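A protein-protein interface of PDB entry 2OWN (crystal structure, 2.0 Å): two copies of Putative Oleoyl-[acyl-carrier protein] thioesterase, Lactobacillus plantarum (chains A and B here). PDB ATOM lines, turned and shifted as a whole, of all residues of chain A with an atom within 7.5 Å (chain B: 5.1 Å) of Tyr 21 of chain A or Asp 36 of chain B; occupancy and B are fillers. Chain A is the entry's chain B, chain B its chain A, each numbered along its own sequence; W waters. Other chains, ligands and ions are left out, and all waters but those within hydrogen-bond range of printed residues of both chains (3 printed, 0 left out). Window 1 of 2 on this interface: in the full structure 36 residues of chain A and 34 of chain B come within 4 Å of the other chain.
Water W3 lies within hydrogen-bond range of the side-chain amide oxygen (OD1) of Asn 180 of chain B (2.7 Å) and the side-chain hydroxyl (OH) of Tyr 20 of chain A (2.7 Å). Water W1 lies within hydrogen-bond range of the backbone carbonyl oxygen of Tyr 21 of chain A (2.8 Å) and the side-chain amide nitrogen of Asn 180 of chain B (3.3 Å). Water W2 bridges OE2 of Glu 22 of chain A (2.8 Å) and OE2 of Glu 22 of chain B (2.8 Å).
Among the printed residues, pairs that only touch across the chains: Arg 17 of chain A with Leu 40 of chain B (3.7 Å), Thr 19 of chain A with Leu 40 of chain B (3.9 Å), Tyr 20 of chain A with Val 39 of chain B (3.3 Å), Tyr 20 of chain A with Leu 40 of chain B (3.7 Å), Tyr 21 of chain A with Asp 36 of chain B (3.5 Å) and Tyr 21 of chain A with Ile 37 of chain B (3.5 Å).
Of the printed residues of chain B, Thr 19 of chain A touches Leu 40. Of chain B, only His 16 (3.1 Å), Glu 22 (2.7 Å), Asp 36 (3.5 Å) and Ile 37 (3.5 Å) come within 4 Å of Tyr 21 of chain A. Gln 78 of chain A touches none of the printed residues of chain B. Of the printed residues of chain A, His 16 of chain B touches Tyr 21. Ile 35 of chain B touches none of the printed residues of chain A. Of chain A, only Tyr 20 and Tyr 21 come within 4 Å of Asp 36 of chain B. Of the printed residues of chain A, Ile 37 of chain B touches Tyr 21. Of the printed residues of chain A, Val 39 of chain B touches Tyr 20. The nearest residue of chain B that does not touch Tyr 21 of chain A is Asn 180 of chain B (4.1 Å). The nearest printed residue of chain B that does not touch Thr 19 of chain A is His 16 of chain B (5.0 Å).
Positions printed for both chains: 16, 22 and 33. Of the 9 pairs that touch across the chains among the printed residues, none has its exchanged pair printed and touching as well.
Printed residues of chain B that touch a printed residue of chain A: His 16, Glu 22, Asp 36, Ile 37, Val 39 and Leu 40. Printed residues of chain A that touch a printed residue of chain B: Arg 17, Thr 19, Tyr 20 and Tyr 21. Hydrophobic or aromatic side chains of chain A that line the printed part of chain B: Tyr 20 and Tyr 21. Among the printed residues, 9 pairs touch across the chains. Among the printed residues, no Asp or Glu carboxylate lies within 4 Å of a Lys or Arg side-chain nitrogen of the other chain.
The side-chain carboxylate (OE1) of Glu 22 of chain B is in hydrogen-bond range of a ring nitrogen (NE2) of His 16 of chain B (2.8 Å). OG1 of Thr 33 of chain B sits at hydrogen-bond distance from O of Glu 22 of chain B, 2.6 Å away. OD1 of Asp 36 of chain B is in hydrogen-bond range of ND2 of Asn 180 of chain B (3.0 Å). The side-chain carboxylate of Glu 22 of chain A sits at hydrogen-bond distance from the backbone NH of Thr 19 of chain A (3.3 Å). O of Thr 19 of chain A sits at hydrogen-bond distance from SG of Cys 23 of chain A (3.4 Å).
A ring nitrogen (NE2) of His 16 of chain B sits close to the side-chain hydroxyl (OH) of Tyr 21 of chain A. OH of Tyr 21 of chain A is in hydrogen-bond range of OE2 of Glu 22 of chain B, 2.7 Å away. The backbone carbonyl oxygen of Asp 36 of chain B is in hydrogen-bond range of the side-chain hydroxyl of Tyr 20 of chain A, at 2.8 Å.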
ATOM      1  N   HIS A  16     -20.825  -5.240 -18.137  1.00  0.00           N
ATOM      2  CA  HIS A  16     -19.404  -5.607 -18.138  1.00  0.00           C
ATOM      3  C   HIS A  16     -18.711  -5.036 -16.901  1.00  0.00           C
ATOM      4  O   HIS A  16     -18.788  -3.830 -16.650  1.00  0.00           O
ATOM      5  CB  HIS A  16     -18.679  -5.122 -19.402  1.00  0.00           C
ATOM      6  CG  HIS A  16     -17.222  -5.488 -19.429  1.00  0.00           C
ATOM      7  ND1 HIS A  16     -16.775  -6.716 -19.859  1.00  0.00           N
ATOM      8  CD2 HIS A  16     -16.123  -4.805 -19.030  1.00  0.00           C
ATOM      9  CE1 HIS A  16     -15.463  -6.772 -19.733  1.00  0.00           C
ATOM     10  NE2 HIS A  16     -15.039  -5.624 -19.235  1.00  0.00           N
ATOM     11  N   ARG A  17     -17.990  -5.912 -16.207  1.00  0.00           N
ATOM     12  CA  ARG A  17     -17.220  -5.584 -15.031  1.00  0.00           C
ATOM     13  C   ARG A  17     -15.840  -5.194 -15.563  1.00  0.00           C
ATOM     14  O   ARG A  17     -15.146  -6.033 -16.171  1.00  0.00           O
ATOM     15  CB  ARG A  17     -17.192  -6.774 -14.054  1.00  0.00           C
ATOM     16  CG  ARG A  17     -16.315  -6.650 -12.837  1.00  0.00           C
ATOM     17  CD  ARG A  17     -14.841  -6.998 -13.086  1.00  0.00           C
ATOM     18  NE  ARG A  17     -14.144  -6.881 -11.838  1.00  0.00           N
ATOM     19  CZ  ARG A  17     -13.998  -7.839 -10.926  1.00  0.00           C
ATOM     20  NH1 ARG A  17     -14.482  -9.097 -11.070  1.00  0.00           N
ATOM     21  NH2 ARG A  17     -13.328  -7.524  -9.839  1.00  0.00           N
ATOM     22  N   ILE A  18     -15.422  -3.960 -15.272  1.00  0.00           N
ATOM     23  CA  ILE A  18     -14.109  -3.434 -15.675  1.00  0.00           C
ATOM     24  C   ILE A  18     -13.086  -4.031 -14.703  1.00  0.00           C
ATOM     25  O   ILE A  18     -13.214  -3.834 -13.492  1.00  0.00           O
ATOM     26  CB  ILE A  18     -14.046  -1.895 -15.621  1.00  0.00           C
ATOM     27  CG1 ILE A  18     -15.075  -1.243 -16.560  1.00  0.00           C
ATOM     28  CG2 ILE A  18     -12.621  -1.354 -15.967  1.00  0.00           C
ATOM     29  CD1 ILE A  18     -14.812  -1.426 -18.058  1.00  0.00           C
ATOM     30  N   THR A  19     -12.125  -4.794 -15.235  1.00  0.00           N
ATOM     31  CA  THR A  19     -11.069  -5.440 -14.441  1.00  0.00           C
ATOM     32  C   THR A  19      -9.854  -4.521 -14.333  1.00  0.00           C
ATOM     33  O   THR A  19      -9.703  -3.600 -15.145  1.00  0.00           O
ATOM     34  CB  THR A  19     -10.628  -6.795 -15.064  1.00  0.00           C
ATOM     35  OG1 THR A  19     -10.047  -6.572 -16.354  1.00  0.00           O
ATOM     36  CG2 THR A  19     -11.819  -7.742 -15.205  1.00  0.00           C
ATOM     37  N   TYR A  20      -8.994  -4.791 -13.342  1.00  0.00           N
ATOM     38  CA  TYR A  20      -7.732  -4.033 -13.122  1.00  0.00           C
ATOM     39  C   TYR A  20      -6.827  -4.062 -14.396  1.00  0.00           C
ATOM     40  O   TYR A  20      -6.205  -3.048 -14.744  1.00  0.00           O
ATOM     41  CB  TYR A  20      -6.961  -4.541 -11.857  1.00  0.00           C
ATOM     42  CG  TYR A  20      -6.309  -5.893 -12.057  1.00  0.00           C
ATOM     43  CD1 TYR A  20      -7.013  -7.091 -11.829  1.00  0.00           C
ATOM     44  CD2 TYR A  20      -4.982  -5.978 -12.585  1.00  0.00           C
ATOM     45  CE1 TYR A  20      -6.407  -8.339 -12.089  1.00  0.00           C
ATOM     46  CE2 TYR A  20      -4.384  -7.206 -12.861  1.00  0.00           C
ATOM     47  CZ  TYR A  20      -5.101  -8.381 -12.606  1.00  0.00           C
ATOM     48  OH  TYR A  20      -4.508  -9.555 -12.855  1.00  0.00           O
ATOM     49  N   TYR A  21      -6.791  -5.229 -15.066  1.00  0.00           N
ATOM     50  CA  TYR A  21      -5.983  -5.454 -16.288  1.00  0.00           C
ATOM     51  C   TYR A  21      -6.521  -4.750 -17.540  1.00  0.00           C
ATOM     52  O   TYR A  21      -5.789  -4.629 -18.515  1.00  0.00           O
ATOM     53  CB  TYR A  21      -5.681  -6.945 -16.534  1.00  0.00           C
ATOM     54  CG  TYR A  21      -6.846  -7.880 -16.763  1.00  0.00           C
ATOM     55  CD1 TYR A  21      -7.340  -8.120 -18.064  1.00  0.00           C
ATOM     56  CD2 TYR A  21      -7.437  -8.571 -15.684  1.00  0.00           C
ATOM     57  CE1 TYR A  21      -8.418  -9.036 -18.285  1.00  0.00           C
ATOM     58  CE2 TYR A  21      -8.512  -9.484 -15.879  1.00  0.00           C
ATOM     59  CZ  TYR A  21      -8.995  -9.709 -17.182  1.00  0.00           C
ATOM     60  OH  TYR A  21     -10.012 -10.604 -17.354  1.00  0.00           O
ATOM     61  N   GLU A  22      -7.792  -4.327 -17.510  1.00  0.00           N
ATOM     62  CA  GLU A  22      -8.412  -3.505 -18.564  1.00  0.00           C
ATOM     63  C   GLU A  22      -8.168  -1.989 -18.308  1.00  0.00           C
ATOM     64  O   GLU A  22      -8.567  -1.161 -19.132  1.00  0.00           O
ATOM     65  CB  GLU A  22      -9.914  -3.790 -18.652  1.00  0.00           C
ATOM     66  CG  GLU A  22     -10.249  -5.145 -19.271  1.00  0.00           C
ATOM     67  CD  GLU A  22     -11.724  -5.539 -19.166  1.00  0.00           C
ATOM     68  OE1 GLU A  22     -12.520  -4.831 -18.513  1.00  0.00           O
ATOM     69  OE2 GLU A  22     -12.090  -6.588 -19.739  1.00  0.00           O
ATOM     70  N   CYS A  23      -7.534  -1.632 -17.177  1.00  0.00           N
ATOM     71  CA  CYS A  23      -7.249  -0.262 -16.778  1.00  0.00           C
ATOM     72  C   CYS A  23      -5.769   0.055 -16.844  1.00  0.00           C
ATOM     73  O   CYS A  23      -4.922  -0.846 -16.859  1.00  0.00           O
ATOM     74  CB  CYS A  23      -7.709  -0.016 -15.329  1.00  0.00           C
ATOM     75  SG  CYS A  23      -9.453  -0.207 -15.083  1.00  0.00           S
ATOM     76  N   ASP A  24      -5.494   1.362 -16.839  1.00  0.00           N
ATOM     77  CA  ASP A  24      -4.136   1.916 -16.839  1.00  0.00           C
ATOM     78  C   ASP A  24      -3.737   2.071 -15.355  1.00  0.00           C
ATOM     79  O   ASP A  24      -4.467   1.611 -14.438  1.00  0.00           O
ATOM     80  CB  ASP A  24      -4.038   3.214 -17.717  1.00  0.00           C
ATOM     81  CG  ASP A  24      -4.884   4.399 -17.225  1.00  0.00           C
ATOM     82  OD1 ASP A  24      -5.190   4.534 -16.033  1.00  0.00           O
ATOM     83  OD2 ASP A  24      -5.235   5.242 -18.084  1.00  0.00           O
ATOM     84  N   THR A  30      -8.705   1.897 -20.271  1.00  0.00           N
ATOM     85  CA  THR A  30      -7.935   2.447 -21.375  1.00  0.00           C
ATOM     86  C   THR A  30      -8.860   2.577 -22.594  1.00  0.00           C
ATOM     87  O   THR A  30      -9.969   2.004 -22.598  1.00  0.00           O
ATOM     88  CB  THR A  30      -6.779   1.514 -21.778  1.00  0.00           C
ATOM     89  OG1 THR A  30      -7.317   0.279 -22.261  1.00  0.00           O
ATOM     90  CG2 THR A  30      -5.827   1.242 -20.586  1.00  0.00           C
ATOM     91  N   THR A  33      -9.495  -0.839 -24.102  1.00  0.00           N
ATOM     92  CA  THR A  33     -10.638  -1.476 -23.391  1.00  0.00           C
ATOM     93  C   THR A  33     -12.006  -0.928 -23.826  1.00  0.00           C
ATOM     94  O   THR A  33     -12.931  -1.714 -23.998  1.00  0.00           O
ATOM     95  CB  THR A  33     -10.518  -1.356 -21.859  1.00  0.00           C
ATOM     96  OG1 THR A  33      -9.401  -2.136 -21.452  1.00  0.00           O
ATOM     97  CG2 THR A  33     -11.807  -1.852 -21.096  1.00  0.00           C
ATOM     98  N   GLN A  78     -11.995   1.033 -12.474  1.00  0.00           N
ATOM     99  CA  GLN A  78     -11.712  -0.372 -12.091  1.00  0.00           C
ATOM    100  C   GLN A  78     -12.837  -0.858 -11.158  1.00  0.00           C
ATOM    101  O   GLN A  78     -13.257  -0.119 -10.262  1.00  0.00           O
ATOM    102  CB  GLN A  78     -10.370  -0.513 -11.364  1.00  0.00           C
ATOM    103  CG  GLN A  78      -9.980  -1.934 -10.932  1.00  0.00           C
ATOM    104  CD  GLN A  78      -8.743  -1.972 -10.049  1.00  0.00           C
ATOM    105  OE1 GLN A  78      -7.860  -1.142 -10.169  1.00  0.00           O
ATOM    106  NE2 GLN A  78      -8.686  -2.944  -9.157  1.00  0.00           N
ATOM    107  N   HIS B  16     -15.933 -16.126 -14.847  1.00  0.00           N
ATOM    108  CA  HIS B  16     -15.371 -15.180 -15.817  1.00  0.00           C
ATOM    109  C   HIS B  16     -15.638 -15.643 -17.251  1.00  0.00           C
ATOM    110  O   HIS B  16     -15.269 -16.766 -17.607  1.00  0.00           O
ATOM    111  CB  HIS B  16     -13.856 -14.993 -15.623  1.00  0.00           C
ATOM    112  CG  HIS B  16     -13.248 -14.035 -16.600  1.00  0.00           C
ATOM    113  ND1 HIS B  16     -13.318 -12.672 -16.431  1.00  0.00           N
ATOM    114  CD2 HIS B  16     -12.633 -14.238 -17.790  1.00  0.00           C
ATOM    115  CE1 HIS B  16     -12.749 -12.075 -17.460  1.00  0.00           C
ATOM    116  NE2 HIS B  16     -12.312 -13.001 -18.294  1.00  0.00           N
ATOM    117  N   GLU B  22      -9.225 -11.184 -24.971  1.00  0.00           N
ATOM    118  CA  GLU B  22      -8.412 -11.966 -24.029  1.00  0.00           C
ATOM    119  C   GLU B  22      -7.774 -13.211 -24.701  1.00  0.00           C
ATOM    120  O   GLU B  22      -6.999 -13.912 -24.047  1.00  0.00           O
ATOM    121  CB  GLU B  22      -9.252 -12.413 -22.826  1.00  0.00           C
ATOM    122  CG  GLU B  22      -9.607 -11.267 -21.904  1.00  0.00           C
ATOM    123  CD  GLU B  22     -10.585 -11.627 -20.794  1.00  0.00           C
ATOM    124  OE1 GLU B  22     -11.213 -12.714 -20.806  1.00  0.00           O
ATOM    125  OE2 GLU B  22     -10.756 -10.776 -19.901  1.00  0.00           O
ATOM    126  N   LEU B  31      -1.508 -16.746 -22.202  1.00  0.00           N
ATOM    127  CA  LEU B  31      -0.850 -16.873 -20.860  1.00  0.00           C
ATOM    128  C   LEU B  31      -1.014 -15.597 -20.032  1.00  0.00           C
ATOM    129  O   LEU B  31      -1.131 -15.672 -18.804  1.00  0.00           O
ATOM    130  CB  LEU B  31       0.645 -17.225 -20.944  1.00  0.00           C
ATOM    131  CG  LEU B  31       1.002 -18.664 -21.263  1.00  0.00           C
ATOM    132  CD1 LEU B  31       2.498 -18.826 -21.508  1.00  0.00           C
ATOM    133  CD2 LEU B  31       0.536 -19.571 -20.113  1.00  0.00           C
ATOM    134  N   THR B  32      -0.983 -14.443 -20.721  1.00  0.00           N
ATOM    135  CA  THR B  32      -1.203 -13.111 -20.129  1.00  0.00           C
ATOM    136  C   THR B  32      -2.588 -13.117 -19.485  1.00  0.00           C
ATOM    137  O   THR B  32      -2.693 -12.815 -18.299  1.00  0.00           O
ATOM    138  CB  THR B  32      -1.056 -11.998 -21.161  1.00  0.00           C
ATOM    139  OG1 THR B  32       0.208 -12.160 -21.821  1.00  0.00           O
ATOM    140  CG2 THR B  32      -1.166 -10.596 -20.506  1.00  0.00           C
ATOM    141  N   THR B  33      -3.610 -13.546 -20.244  1.00  0.00           N
ATOM    142  CA  THR B  33      -5.000 -13.679 -19.740  1.00  0.00           C
ATOM    143  C   THR B  33      -5.132 -14.653 -18.564  1.00  0.00           C
ATOM    144  O   THR B  33      -5.842 -14.336 -17.604  1.00  0.00           O
ATOM    145  CB  THR B  33      -6.004 -14.070 -20.861  1.00  0.00           C
ATOM    146  OG1 THR B  33      -6.114 -12.960 -21.748  1.00  0.00           O
ATOM    147  CG2 THR B  33      -7.409 -14.421 -20.304  1.00  0.00           C
ATOM    148  N   LEU B  34      -4.459 -15.807 -18.648  1.00  0.00           N
ATOM    149  CA  LEU B  34      -4.492 -16.849 -17.590  1.00  0.00           C
ATOM    150  C   LEU B  34      -4.038 -16.274 -16.229  1.00  0.00           C
ATOM    151  O   LEU B  34      -4.746 -16.424 -15.231  1.00  0.00           O
ATOM    152  CB  LEU B  34      -3.644 -18.077 -17.972  1.00  0.00           C
ATOM    153  CG  LEU B  34      -3.747 -19.334 -17.095  1.00  0.00           C
ATOM    154  CD1 LEU B  34      -5.137 -19.926 -17.218  1.00  0.00           C
ATOM    155  CD2 LEU B  34      -2.721 -20.357 -17.523  1.00  0.00           C
ATOM    156  N   ILE B  35      -2.898 -15.579 -16.234  1.00  0.00           N
ATOM    157  CA  ILE B  35      -2.364 -14.910 -15.023  1.00  0.00           C
ATOM    158  C   ILE B  35      -3.280 -13.744 -14.598  1.00  0.00           C
ATOM    159  O   ILE B  35      -3.519 -13.576 -13.398  1.00  0.00           O
ATOM    160  CB  ILE B  35      -0.899 -14.428 -15.198  1.00  0.00           C
ATOM    161  CG1 ILE B  35       0.044 -15.612 -15.440  1.00  0.00           C
ATOM    162  CG2 ILE B  35      -0.394 -13.628 -13.982  1.00  0.00           C
ATOM    163  CD1 ILE B  35       0.073 -16.687 -14.390  1.00  0.00           C
ATOM    164  N   ASP B  36      -3.743 -12.947 -15.571  1.00  0.00           N
ATOM    165  CA  ASP B  36      -4.680 -11.823 -15.324  1.00  0.00           C
ATOM    166  C   ASP B  36      -5.920 -12.246 -14.532  1.00  0.00           C
ATOM    167  O   ASP B  36      -6.249 -11.607 -13.529  1.00  0.00           O
ATOM    168  CB  ASP B  36      -5.151 -11.145 -16.637  1.00  0.00           C
ATOM    169  CG  ASP B  36      -4.153 -10.165 -17.231  1.00  0.00           C
ATOM    170  OD1 ASP B  36      -3.283  -9.610 -16.531  1.00  0.00           O
ATOM    171  OD2 ASP B  36      -4.312  -9.910 -18.437  1.00  0.00           O
ATOM    172  N   ILE B  37      -6.546 -13.343 -14.965  1.00  0.00           N
ATOM    173  CA  ILE B  37      -7.772 -13.871 -14.301  1.00  0.00           C
ATOM    174  C   ILE B  37      -7.452 -14.570 -12.964  1.00  0.00           C
ATOM    175  O   ILE B  37      -8.291 -14.518 -12.057  1.00  0.00           O
ATOM    176  CB  ILE B  37      -8.687 -14.697 -15.252  1.00  0.00           C
ATOM    177  CG1 ILE B  37      -8.103 -16.071 -15.632  1.00  0.00           C
ATOM    178  CG2 ILE B  37      -9.028 -13.827 -16.469  1.00  0.00           C
ATOM    179  CD1 ILE B  37      -9.022 -16.879 -16.536  1.00  0.00           C
ATOM    180  N   ALA B  38      -6.281 -15.229 -12.860  1.00  0.00           N
ATOM    181  CA  ALA B  38      -5.810 -15.856 -11.599  1.00  0.00           C
ATOM    182  C   ALA B  38      -5.690 -14.767 -10.524  1.00  0.00           C
ATOM    183  O   ALA B  38      -6.300 -14.868  -9.464  1.00  0.00           O
ATOM    184  CB  ALA B  38      -4.450 -16.557 -11.774  1.00  0.00           C
ATOM    185  N   VAL B  39      -4.958 -13.707 -10.861  1.00  0.00           N
ATOM    186  CA  VAL B  39      -4.741 -12.545  -9.977  1.00  0.00           C
ATOM    187  C   VAL B  39      -6.053 -11.781  -9.677  1.00  0.00           C
ATOM    188  O   VAL B  39      -6.198 -11.267  -8.559  1.00  0.00           O
ATOM    189  CB  VAL B  39      -3.563 -11.653 -10.499  1.00  0.00           C
ATOM    190  CG1 VAL B  39      -3.468 -10.299  -9.775  1.00  0.00           C
ATOM    191  CG2 VAL B  39      -2.251 -12.433 -10.393  1.00  0.00           C
ATOM    192  N   LEU B  40      -6.981 -11.721 -10.655  1.00  0.00           N
ATOM    193  CA  LEU B  40      -8.320 -11.098 -10.477  1.00  0.00           C
ATOM    194  C   LEU B  40      -9.061 -11.764  -9.320  1.00  0.00           C
ATOM    195  O   LEU B  40      -9.579 -11.070  -8.453  1.00  0.00           O
ATOM    196  CB  LEU B  40      -9.186 -11.205 -11.743  1.00  0.00           C
ATOM    197  CG  LEU B  40     -10.569 -10.562 -11.797  1.00  0.00           C
ATOM    198  CD1 LEU B  40     -10.495  -9.051 -11.633  1.00  0.00           C
ATOM    199  CD2 LEU B  40     -11.248 -10.935 -13.122  1.00  0.00           C
ATOM    200  N   ASN B 180       2.565  -4.957 -14.747  1.00  0.00           N
ATOM    201  CA  ASN B 180       1.737  -6.129 -14.564  1.00  0.00           C
ATOM    202  C   ASN B 180       2.611  -7.293 -15.052  1.00  0.00           C
ATOM    203  O   ASN B 180       2.932  -7.354 -16.248  1.00  0.00           O
ATOM    204  CB  ASN B 180       0.414  -6.019 -15.349  1.00  0.00           C
ATOM    205  CG  ASN B 180      -0.496  -7.266 -15.258  1.00  0.00           C
ATOM    206  OD1 ASN B 180      -0.149  -8.280 -14.663  1.00  0.00           O
ATOM    207  ND2 ASN B 180      -1.680  -7.180 -15.902  1.00  0.00           N
ATOM    208  N   ALA B 182       1.876 -10.266 -15.655  1.00  0.00           N
ATOM    209  CA  ALA B 182       1.181 -10.976 -16.744  1.00  0.00           C
ATOM    210  C   ALA B 182       1.695 -10.534 -18.123  1.00  0.00           C
ATOM    211  O   ALA B 182       1.894 -11.385 -18.988  1.00  0.00           O
ATOM    212  CB  ALA B 182      -0.349 -10.798 -16.650  1.00  0.00           C
HETATM  213  O   HOH W   1      -3.091  -4.953 -17.927  1.00  0.00           O
HETATM  214  O   HOH W   2     -13.037  -9.203 -19.238  1.00  0.00           O
HETATM  215  O   HOH W   3      -1.833  -9.750 -13.239  1.00  0.00           O
